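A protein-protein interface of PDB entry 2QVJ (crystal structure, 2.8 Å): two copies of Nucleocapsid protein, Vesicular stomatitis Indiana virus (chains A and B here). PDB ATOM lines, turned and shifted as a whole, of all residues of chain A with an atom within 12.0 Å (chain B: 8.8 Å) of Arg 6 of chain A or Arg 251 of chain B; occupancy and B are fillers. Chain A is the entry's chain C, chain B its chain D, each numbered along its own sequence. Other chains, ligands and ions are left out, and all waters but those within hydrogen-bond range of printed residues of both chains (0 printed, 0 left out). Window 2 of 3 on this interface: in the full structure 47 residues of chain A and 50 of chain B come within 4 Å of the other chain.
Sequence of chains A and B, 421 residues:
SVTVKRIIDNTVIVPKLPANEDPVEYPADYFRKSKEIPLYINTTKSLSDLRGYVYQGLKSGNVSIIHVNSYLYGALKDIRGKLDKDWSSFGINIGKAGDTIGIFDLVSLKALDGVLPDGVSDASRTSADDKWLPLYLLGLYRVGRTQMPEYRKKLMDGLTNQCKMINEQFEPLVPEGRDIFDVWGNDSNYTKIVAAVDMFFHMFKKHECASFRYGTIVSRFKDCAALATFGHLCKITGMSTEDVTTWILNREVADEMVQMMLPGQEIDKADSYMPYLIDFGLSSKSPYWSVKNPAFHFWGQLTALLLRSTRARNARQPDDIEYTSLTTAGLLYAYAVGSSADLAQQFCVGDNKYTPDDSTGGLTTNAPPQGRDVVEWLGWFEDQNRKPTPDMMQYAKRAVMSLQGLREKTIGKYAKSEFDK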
ATOM      1  N   VAL A   2       5.849 -33.258  -9.696  1.00  0.00           N
ATOM      2  CA  VAL A   2       7.085 -32.557 -10.034  1.00  0.00           C
ATOM      3  C   VAL A   2       7.294 -31.367  -9.092  1.00  0.00           C
ATOM      4  O   VAL A   2       8.423 -31.099  -8.670  1.00  0.00           O
ATOM      5  CB  VAL A   2       7.106 -32.087 -11.522  1.00  0.00           C
ATOM      6  CG1 VAL A   2       8.495 -31.594 -11.920  1.00  0.00           C
ATOM      7  CG2 VAL A   2       6.670 -33.213 -12.454  1.00  0.00           C
ATOM      8  N   THR A   3       6.203 -30.677  -8.757  1.00  0.00           N
ATOM      9  CA  THR A   3       6.265 -29.464  -7.932  1.00  0.00           C
ATOM     10  C   THR A   3       5.591 -29.620  -6.568  1.00  0.00           C
ATOM     11  O   THR A   3       4.423 -30.003  -6.478  1.00  0.00           O
ATOM     12  CB  THR A   3       5.670 -28.237  -8.666  1.00  0.00           C
ATOM     13  OG1 THR A   3       4.419 -28.594  -9.263  1.00  0.00           O
ATOM     14  CG2 THR A   3       6.625 -27.743  -9.753  1.00  0.00           C
ATOM     15  N   VAL A   4       6.343 -29.311  -5.513  1.00  0.00           N
ATOM     16  CA  VAL A   4       5.861 -29.438  -4.136  1.00  0.00           C
ATOM     17  C   VAL A   4       5.608 -28.059  -3.521  1.00  0.00           C
ATOM     18  O   VAL A   4       6.434 -27.152  -3.643  1.00  0.00           O
ATOM     19  CB  VAL A   4       6.862 -30.232  -3.244  1.00  0.00           C
ATOM     20  CG1 VAL A   4       6.248 -30.558  -1.890  1.00  0.00           C
ATOM     21  CG2 VAL A   4       7.304 -31.512  -3.934  1.00  0.00           C
ATOM     22  N   LYS A   5       4.457 -27.913  -2.867  1.00  0.00           N
ATOM     23  CA  LYS A   5       4.115 -26.683  -2.151  1.00  0.00           C
ATOM     24  C   LYS A   5       4.052 -26.945  -0.647  1.00  0.00           C
ATOM     25  O   LYS A   5       3.680 -28.038  -0.213  1.00  0.00           O
ATOM     26  CB  LYS A   5       2.773 -26.103  -2.629  1.00  0.00           C
ATOM     27  CG  LYS A   5       2.524 -26.136  -4.138  1.00  0.00           C
ATOM     28  CD  LYS A   5       1.624 -27.312  -4.546  1.00  0.00           C
ATOM     29  CE  LYS A   5       0.149 -27.046  -4.214  1.00  0.00           C
ATOM     30  NZ  LYS A   5      -0.729 -28.231  -4.459  1.00  0.00           N
ATOM     31  N   ARG A   6       4.426 -25.936   0.137  1.00  0.00           N
ATOM     32  CA  ARG A   6       4.301 -25.981   1.591  1.00  0.00           C
ATOM     33  C   ARG A   6       2.955 -25.371   1.979  1.00  0.00           C
ATOM     34  O   ARG A   6       2.714 -24.188   1.724  1.00  0.00           O
ATOM     35  CB  ARG A   6       5.452 -25.210   2.239  1.00  0.00           C
ATOM     36  CG  ARG A   6       5.611 -25.435   3.732  1.00  0.00           C
ATOM     37  CD  ARG A   6       6.740 -24.584   4.281  1.00  0.00           C
ATOM     38  NE  ARG A   6       6.929 -24.779   5.716  1.00  0.00           N
ATOM     39  CZ  ARG A   6       7.786 -24.090   6.463  1.00  0.00           C
ATOM     40  NH1 ARG A   6       8.547 -23.144   5.921  1.00  0.00           N
ATOM     41  NH2 ARG A   6       7.883 -24.343   7.760  1.00  0.00           N
ATOM     42  N   ILE A   7       2.091 -26.179   2.597  1.00  0.00           N
ATOM     43  CA  ILE A   7       0.676 -25.816   2.823  1.00  0.00           C
ATOM     44  C   ILE A   7       0.443 -24.484   3.539  1.00  0.00           C
ATOM     45  O   ILE A   7      -0.536 -23.791   3.263  1.00  0.00           O
ATOM     46  CB  ILE A   7      -0.136 -26.959   3.518  1.00  0.00           C
ATOM     47  CG1 ILE A   7       0.420 -27.297   4.908  1.00  0.00           C
ATOM     48  CG2 ILE A   7      -0.183 -28.206   2.643  1.00  0.00           C
ATOM     49  CD1 ILE A   7      -0.377 -26.714   6.065  1.00  0.00           C
ATOM     50  N   ILE A   8       1.354 -24.136   4.445  1.00  0.00           N
ATOM     51  CA  ILE A   8       1.203 -22.970   5.316  1.00  0.00           C
ATOM     52  C   ILE A   8       1.251 -21.646   4.543  1.00  0.00           C
ATOM     53  O   ILE A   8       0.363 -20.801   4.692  1.00  0.00           O
ATOM     54  CB  ILE A   8       2.262 -22.968   6.466  1.00  0.00           C
ATOM     55  CG1 ILE A   8       2.216 -24.274   7.269  1.00  0.00           C
ATOM     56  CG2 ILE A   8       2.049 -21.790   7.409  1.00  0.00           C
ATOM     57  CD1 ILE A   8       3.182 -25.354   6.791  1.00  0.00           C
ATOM     58  N   ASP A   9       2.279 -21.484   3.715  1.00  0.00           N
ATOM     59  CA  ASP A   9       2.530 -20.222   3.017  1.00  0.00           C
ATOM     60  C   ASP A   9       2.548 -20.344   1.487  1.00  0.00           C
ATOM     61  O   ASP A   9       2.951 -19.406   0.792  1.00  0.00           O
ATOM     62  CB  ASP A   9       3.833 -19.590   3.523  1.00  0.00           C
ATOM     63  CG  ASP A   9       4.984 -20.586   3.600  1.00  0.00           C
ATOM     64  OD1 ASP A   9       5.739 -20.536   4.594  1.00  0.00           O
ATOM     65  OD2 ASP A   9       5.138 -21.418   2.679  1.00  0.00           O
ATOM     66  N   ASN A  10       2.122 -21.502   0.978  1.00  0.00           N
ATOM     67  CA  ASN A  10       1.991 -21.757  -0.468  1.00  0.00           C
ATOM     68  C   ASN A  10       3.315 -21.777  -1.251  1.00  0.00           C
ATOM     69  O   ASN A  10       3.326 -22.052  -2.453  1.00  0.00           O
ATOM     70  CB  ASN A  10       0.982 -20.775  -1.099  1.00  0.00           C
ATOM     71  CG  ASN A  10       0.600 -21.148  -2.525  1.00  0.00           C
ATOM     72  OD1 ASN A  10       0.289 -22.303  -2.821  1.00  0.00           O
ATOM     73  ND2 ASN A  10       0.615 -20.162  -3.414  1.00  0.00           N
ATOM     74  N   THR A  11       4.424 -21.507  -0.565  1.00  0.00           N
ATOM     75  CA  THR A  11       5.742 -21.420  -1.205  1.00  0.00           C
ATOM     76  C   THR A  11       6.167 -22.751  -1.834  1.00  0.00           C
ATOM     77  O   THR A  11       5.840 -23.824  -1.323  1.00  0.00           O
ATOM     78  CB  THR A  11       6.826 -20.938  -0.212  1.00  0.00           C
ATOM     79  OG1 THR A  11       6.273 -19.953   0.667  1.00  0.00           O
ATOM     80  CG2 THR A  11       8.013 -20.331  -0.954  1.00  0.00           C
ATOM     81  N   VAL A  12       6.885 -22.661  -2.952  1.00  0.00           N
ATOM     82  CA  VAL A  12       7.378 -23.831  -3.676  1.00  0.00           C
ATOM     83  C   VAL A  12       8.717 -24.297  -3.104  1.00  0.00           C
ATOM     84  O   VAL A  12       9.618 -23.491  -2.864  1.00  0.00           O
ATOM     85  CB  VAL A  12       7.504 -23.545  -5.200  1.00  0.00           C
ATOM     86  CG1 VAL A  12       8.251 -24.663  -5.921  1.00  0.00           C
ATOM     87  CG2 VAL A  12       6.124 -23.347  -5.821  1.00  0.00           C
ATOM     88  N   ILE A  13       8.827 -25.603  -2.881  1.00  0.00           N
ATOM     89  CA  ILE A  13      10.061 -26.217  -2.401  1.00  0.00           C
ATOM     90  C   ILE A  13      10.528 -27.308  -3.371  1.00  0.00           C
ATOM     91  O   ILE A  13       9.738 -28.150  -3.797  1.00  0.00           O
ATOM     92  CB  ILE A  13       9.900 -26.766  -0.949  1.00  0.00           C
ATOM     93  CG1 ILE A  13      11.199 -27.429  -0.463  1.00  0.00           C
ATOM     94  CG2 ILE A  13       8.684 -27.704  -0.841  1.00  0.00           C
ATOM     95  CD1 ILE A  13      11.234 -27.748   1.025  1.00  0.00           C
ATOM     96  N   VAL A  14      11.811 -27.275  -3.723  1.00  0.00           N
ATOM     97  CA  VAL A  14      12.393 -28.259  -4.636  1.00  0.00           C
ATOM     98  C   VAL A  14      13.278 -29.238  -3.862  1.00  0.00           C
ATOM     99  O   VAL A  14      14.390 -28.881  -3.467  1.00  0.00           O
ATOM    100  CB  VAL A  14      13.222 -27.592  -5.764  1.00  0.00           C
ATOM    101  CG1 VAL A  14      13.558 -28.608  -6.847  1.00  0.00           C
ATOM    102  CG2 VAL A  14      12.479 -26.405  -6.362  1.00  0.00           C
ATOM    103  N   PRO A  15      12.783 -30.470  -3.630  1.00  0.00           N
ATOM    104  CA  PRO A  15      13.564 -31.506  -2.962  1.00  0.00           C
ATOM    105  C   PRO A  15      14.709 -32.003  -3.839  1.00  0.00           C
ATOM    106  O   PRO A  15      14.474 -32.512  -4.938  1.00  0.00           O
ATOM    107  CB  PRO A  15      12.540 -32.627  -2.726  1.00  0.00           C
ATOM    108  CG  PRO A  15      11.204 -31.998  -2.930  1.00  0.00           C
ATOM    109  CD  PRO A  15      11.434 -30.953  -3.964  1.00  0.00           C
ATOM    110  N   THR B 245       9.000 -36.172   1.223  1.00  0.00           N
ATOM    111  CA  THR B 245       8.780 -34.810   1.715  1.00  0.00           C
ATOM    112  C   THR B 245       7.347 -34.593   2.226  1.00  0.00           C
ATOM    113  O   THR B 245       7.148 -33.930   3.244  1.00  0.00           O
ATOM    114  CB  THR B 245       9.137 -33.765   0.633  1.00  0.00           C
ATOM    115  OG1 THR B 245      10.494 -33.963   0.219  1.00  0.00           O
ATOM    116  CG2 THR B 245       8.983 -32.340   1.159  1.00  0.00           C
ATOM    117  N   THR B 246       6.363 -35.163   1.531  1.00  0.00           N
ATOM    118  CA  THR B 246       4.956 -35.061   1.947  1.00  0.00           C
ATOM    119  C   THR B 246       4.651 -35.819   3.240  1.00  0.00           C
ATOM    120  O   THR B 246       3.592 -35.621   3.838  1.00  0.00           O
ATOM    121  CB  THR B 246       3.979 -35.551   0.853  1.00  0.00           C
ATOM    122  OG1 THR B 246       4.272 -36.915   0.520  1.00  0.00           O
ATOM    123  CG2 THR B 246       4.066 -34.678  -0.396  1.00  0.00           C
ATOM    124  N   ILE B 248       6.431 -35.535   5.995  1.00  0.00           N
ATOM    125  CA  ILE B 248       6.815 -34.702   7.128  1.00  0.00           C
ATOM    126  C   ILE B 248       5.544 -34.200   7.816  1.00  0.00           C
ATOM    127  O   ILE B 248       4.701 -33.551   7.189  1.00  0.00           O
ATOM    128  CB  ILE B 248       7.718 -33.521   6.692  1.00  0.00           C
ATOM    129  CG1 ILE B 248       9.083 -34.040   6.224  1.00  0.00           C
ATOM    130  CG2 ILE B 248       7.886 -32.512   7.828  1.00  0.00           C
ATOM    131  CD1 ILE B 248       9.969 -32.990   5.579  1.00  0.00           C
ATOM    132  N   LEU B 249       5.408 -34.513   9.102  1.00  0.00           N
ATOM    133  CA  LEU B 249       4.171 -34.240   9.832  1.00  0.00           C
ATOM    134  C   LEU B 249       4.350 -33.300  11.032  1.00  0.00           C
ATOM    135  O   LEU B 249       3.389 -33.011  11.746  1.00  0.00           O
ATOM    136  CB  LEU B 249       3.514 -35.558  10.263  1.00  0.00           C
ATOM    137  CG  LEU B 249       3.294 -36.633   9.188  1.00  0.00           C
ATOM    138  CD1 LEU B 249       2.852 -37.954   9.806  1.00  0.00           C
ATOM    139  CD2 LEU B 249       2.297 -36.176   8.128  1.00  0.00           C
ATOM    140  N   ASN B 250       5.578 -32.830  11.248  1.00  0.00           N
ATOM    141  CA  ASN B 250       5.875 -31.893  12.328  1.00  0.00           C
ATOM    142  C   ASN B 250       6.393 -30.574  11.763  1.00  0.00           C
ATOM    143  O   ASN B 250       7.214 -30.569  10.846  1.00  0.00           O
ATOM    144  CB  ASN B 250       6.891 -32.489  13.310  1.00  0.00           C
ATOM    145  CG  ASN B 250       6.549 -33.915  13.729  1.00  0.00           C
ATOM    146  OD1 ASN B 250       5.896 -34.138  14.750  1.00  0.00           O
ATOM    147  ND2 ASN B 250       6.992 -34.887  12.937  1.00  0.00           N
ATOM    148  N   ARG B 251       5.911 -29.462  12.316  1.00  0.00           N
ATOM    149  CA  ARG B 251       6.207 -28.117  11.798  1.00  0.00           C
ATOM    150  C   ARG B 251       7.693 -27.748  11.831  1.00  0.00           C
ATOM    151  O   ARG B 251       8.195 -27.094  10.913  1.00  0.00           O
ATOM    152  CB  ARG B 251       5.364 -27.064  12.537  1.00  0.00           C
ATOM    153  CG  ARG B 251       5.755 -25.599  12.308  1.00  0.00           C
ATOM    154  CD  ARG B 251       5.396 -25.108  10.911  1.00  0.00           C
ATOM    155  NE  ARG B 251       5.854 -23.737  10.684  1.00  0.00           N
ATOM    156  CZ  ARG B 251       5.092 -22.652  10.807  1.00  0.00           C
ATOM    157  NH1 ARG B 251       3.814 -22.761  11.151  1.00  0.00           N
ATOM    158  NH2 ARG B 251       5.610 -21.451  10.580  1.00  0.00           N
ATOM    159  N   GLU B 252       8.392 -28.173  12.881  1.00  0.00           N
ATOM    160  CA  GLU B 252       9.807 -27.844  13.050  1.00  0.00           C
ATOM    161  C   GLU B 252      10.692 -28.626  12.079  1.00  0.00           C
ATOM    162  O   GLU B 252      11.793 -28.184  11.746  1.00  0.00           O
ATOM    163  CB  GLU B 252      10.244 -28.079  14.500  1.00  0.00           C
ATOM    164  CG  GLU B 252      11.141 -26.982  15.070  1.00  0.00           C
ATOM    165  CD  GLU B 252      12.621 -27.282  14.924  1.00  0.00           C
ATOM    166  OE1 GLU B 252      13.106 -28.221  15.593  1.00  0.00           O
ATOM    167  OE2 GLU B 252      13.306 -26.570  14.157  1.00  0.00           O
ATOM    168  N   VAL B 253      10.206 -29.782  11.630  1.00  0.00           N
ATOM    169  CA  VAL B 253      10.898 -30.576  10.617  1.00  0.00           C
ATOM    170  C   VAL B 253      10.752 -29.893   9.262  1.00  0.00           C
ATOM    171  O   VAL B 253      11.696 -29.863   8.472  1.00  0.00           O
ATOM    172  CB  VAL B 253      10.362 -32.028  10.542  1.00  0.00           C
ATOM    173  CG1 VAL B 253      11.198 -32.871   9.585  1.00  0.00           C
ATOM    174  CG2 VAL B 253      10.356 -32.665  11.915  1.00  0.00           C
ATOM    175  N   ALA B 254       9.566 -29.337   9.013  1.00  0.00           N
ATOM    176  CA  ALA B 254       9.284 -28.587   7.790  1.00  0.00           C
ATOM    177  C   ALA B 254      10.218 -27.390   7.636  1.00  0.00           C
ATOM    178  O   ALA B 254      10.754 -27.164   6.555  1.00  0.00           O
ATOM    179  CB  ALA B 254       7.833 -28.140   7.762  1.00  0.00           C
ATOM    180  N   ASP B 255      10.413 -26.639   8.721  1.00  0.00           N
ATOM    181  CA  ASP B 255      11.353 -25.515   8.745  1.00  0.00           C
ATOM    182  C   ASP B 255      12.759 -25.947   8.335  1.00  0.00           C
ATOM    183  O   ASP B 255      13.437 -25.248   7.578  1.00  0.00           O
ATOM    184  CB  ASP B 255      11.407 -24.870  10.139  1.00  0.00           C
ATOM    185  CG  ASP B 255      10.155 -24.075  10.475  1.00  0.00           C
ATOM    186  OD1 ASP B 255       9.605 -23.392   9.583  1.00  0.00           O
ATOM    187  OD2 ASP B 255       9.728 -24.122  11.652  1.00  0.00           O
ATOM    188  N   GLU B 256      13.180 -27.106   8.835  1.00  0.00           N
ATOM    189  CA  GLU B 256      14.513 -27.638   8.569  1.00  0.00           C
ATOM    190  C   GLU B 256      14.699 -28.082   7.119  1.00  0.00           C
ATOM    191  O   GLU B 256      15.787 -27.936   6.558  1.00  0.00           O
ATOM    192  CB  GLU B 256      14.833 -28.778   9.541  1.00  0.00           C
ATOM    193  CG  GLU B 256      15.121 -28.290  10.958  1.00  0.00           C
ATOM    194  CD  GLU B 256      15.003 -29.377  12.011  1.00  0.00           C
ATOM    195  OE1 GLU B 256      14.721 -29.032  13.178  1.00  0.00           O
ATOM    196  OE2 GLU B 256      15.191 -30.570  11.683  1.00  0.00           O
ATOM    197  N   MET B 257      13.636 -28.609   6.513  1.00  0.00           N
ATOM    198  CA  MET B 257      13.672 -29.015   5.109  1.00  0.00           C
ATOM    199  C   MET B 257      13.795 -27.800   4.181  1.00  0.00           C
ATOM    200  O   MET B 257      14.578 -27.819   3.230  1.00  0.00           O
ATOM    201  CB  MET B 257      12.447 -29.866   4.756  1.00  0.00           C
ATOM    202  CG  MET B 257      12.520 -30.567   3.400  1.00  0.00           C
ATOM    203  SD  MET B 257      14.005 -31.574   3.156  1.00  0.00           S
ATOM    204  CE  MET B 257      13.699 -32.937   4.280  1.00  0.00           C
ATOM    205  N   VAL B 258      13.030 -26.751   4.476  1.00  0.00           N
ATOM    206  CA  VAL B 258      13.106 -25.474   3.758  1.00  0.00           C
ATOM    207  C   VAL B 258      14.507 -24.855   3.875  1.00  0.00           C
ATOM    208  O   VAL B 258      15.054 -24.346   2.891  1.00  0.00           O
ATOM    209  CB  VAL B 258      12.017 -24.481   4.261  1.00  0.00           C
ATOM    210  CG1 VAL B 258      12.192 -23.095   3.639  1.00  0.00           C
ATOM    211  CG2 VAL B 258      10.627 -25.024   3.957  1.00  0.00           C
ATOM    212  N   GLN B 259      15.075 -24.916   5.079  1.00  0.00           N
ATOM    213  CA  GLN B 259      16.437 -24.455   5.346  1.00  0.00           C
ATOM    214  C   GLN B 259      17.457 -25.238   4.514  1.00  0.00           C
ATOM    215  O   GLN B 259      18.404 -24.660   3.971  1.00  0.00           O
ATOM    216  CB  GLN B 259      16.748 -24.571   6.845  1.00  0.00           C
ATOM    217  CG  GLN B 259      18.134 -24.077   7.265  1.00  0.00           C
ATOM    218  CD  GLN B 259      18.305 -23.998   8.778  1.00  0.00           C
ATOM    219  OE1 GLN B 259      19.027 -24.797   9.377  1.00  0.00           O
ATOM    220  NE2 GLN B 259      17.639 -23.031   9.400  1.00  0.00           N
ATOM    221  N   ALA B 295      15.416 -32.046  14.628  1.00  0.00           N
ATOM    222  CA  ALA B 295      14.130 -32.726  14.495  1.00  0.00           C
ATOM    223  C   ALA B 295      14.132 -33.714  13.329  1.00  0.00           C
ATOM    224  O   ALA B 295      13.665 -34.845  13.469  1.00  0.00           O
ATOM    225  CB  ALA B 295      13.007 -31.711  14.340  1.00  0.00           C
ATOM    226  N   GLU B 322      10.775 -32.391  20.120  1.00  0.00           N
ATOM    227  CA  GLU B 322       9.545 -33.035  20.562  1.00  0.00           C
ATOM    228  C   GLU B 322       9.585 -34.538  20.278  1.00  0.00           C
ATOM    229  O   GLU B 322       8.997 -35.015  19.302  1.00  0.00           O
ATOM    230  CB  GLU B 322       8.318 -32.373  19.930  1.00  0.00           C
ATOM    231  CG  GLU B 322       7.028 -32.613  20.720  1.00  0.00           C
ATOM    232  CD  GLU B 322       5.804 -31.951  20.102  1.00  0.00           C
ATOM    233  OE1 GLU B 322       5.942 -31.246  19.076  1.00  0.00           O
ATOM    234  OE2 GLU B 322       4.695 -32.146  20.647  1.00  0.00           O
ATOM    235  N   SER B 325       6.092 -36.652  19.669  1.00  0.00           N
ATOM    236  CA  SER B 325       5.412 -36.371  18.396  1.00  0.00           C
ATOM    237  C   SER B 325       6.180 -36.941  17.211  1.00  0.00           C
ATOM    238  O   SER B 325       5.583 -37.514  16.299  1.00  0.00           O
ATOM    239  CB  SER B 325       5.196 -34.870  18.200  1.00  0.00           C
ATOM    240  OG  SER B 325       4.206 -34.375  19.077  1.00  0.00           O
ATOM    241  N   LEU B 326       7.502 -36.776  17.242  1.00  0.00           N
ATOM    242  CA  LEU B 326       8.395 -37.292  16.209  1.00  0.00           C
ATOM    243  C   LEU B 326       8.370 -38.812  16.148  1.00  0.00           C
ATOM    244  O   LEU B 326       8.398 -39.393  15.064  1.00  0.00           O
ATOM    245  CB  LEU B 326       9.827 -36.812  16.458  1.00  0.00           C
ATOM    246  CG  LEU B 326      10.152 -35.349  16.153  1.00  0.00           C
ATOM    247  CD1 LEU B 326      11.366 -34.896  16.933  1.00  0.00           C
ATOM    248  CD2 LEU B 326      10.362 -35.138  14.664  1.00  0.00           C
ATOM    249  N   ALA B 329       4.956 -39.834  14.584  1.00  0.00           N
ATOM    250  CA  ALA B 329       5.075 -39.510  13.163  1.00  0.00           C
ATOM    251  C   ALA B 329       5.993 -40.496  12.441  1.00  0.00           C
ATOM    252  O   ALA B 329       5.654 -41.003  11.370  1.00  0.00           O
ATOM    253  CB  ALA B 329       5.587 -38.090  12.986  1.00  0.00           C
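Thr 3 of chain A touches none of the printed residues of chain B. Of chain B, only Arg 251, Ala 254, Asp 255 and Val 258 come within 4 Å of Arg 6 of chain A. Of the printed residues of chain B, Ile 13 of chain A touches Met 257. Printed residues of chain B within 4 Å of Pro 15 of chain A: Thr 245. Of the printed residues of chain A, Thr 245 of chain B touches Pro 15. No residue of chain A comes within 4 Å of Asn 250 of chain B. Of chain A, only Arg 6 (3.6 Å) comes within 4 Å of Arg 251 of chain B. No residue of chain A comes within 4 Å of Glu 252 of chain B. No residue of chain A comes within 4 Å of Val 253 of chain B. Of chain A, only Arg 6 comes within 4 Å of Ala 254 of chain B. Asp 255 of chain B touches one residue of chain A. Of the printed residues of chain A, Met 257 of chain B touches Ile 13 (3.9 Å). Of the printed residues of chain A, Val 258 of chain B touches Arg 6. The nearest residue of chain B that does not touch Arg 6 of chain A is Glu 256 of chain B (6.1 Å). The nearest printed residue of chain B that does not touch Ile 13 of chain A is Val 258 of chain B (4.02 Å).
Arg 251 of chain B touches Arg 6 of chain A (NE to NH2, 3.6 Å). Ala 254 of chain B touches Arg 6 of chain A (CB to NH2, 3.8 Å). NH1 of Arg 6 of chain A touches CG2 of Val 258 of chain B (3.4 Å). Met 257 of chain B touches Ile 13 of chain A (CG to CD1, 3.9 Å). Pro 15 of chain A touches Thr 245 of chain B (CG to OG1, 3.8 Å).
No position is printed for both chains.
OD1 of Asp 255 of chain B is in salt-bridge range of NE of Arg 251 of chain B (3.9 Å). O of Val 4 of chain A sits at hydrogen-bond distance from N of Ile 13 of chain A, 3.0 Å away. N of Arg 6 of chain A sits at hydrogen-bond distance from O of Thr 11 of chain A (2.9 Å).
OD1 of Asp 255 of chain B is in salt-bridge range of NH2 of Arg 6 of chain A (2.7 Å).
Hydrophobic or aromatic side chains of chain A within 4 Å of the printed part of chain B: Ile 13 and Pro 15. Of the 19 printed residues of chain B, 6 touch a printed residue of chain A. Along chain B the printed residues that touch a printed residue of chain A span positions 245 to 258.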
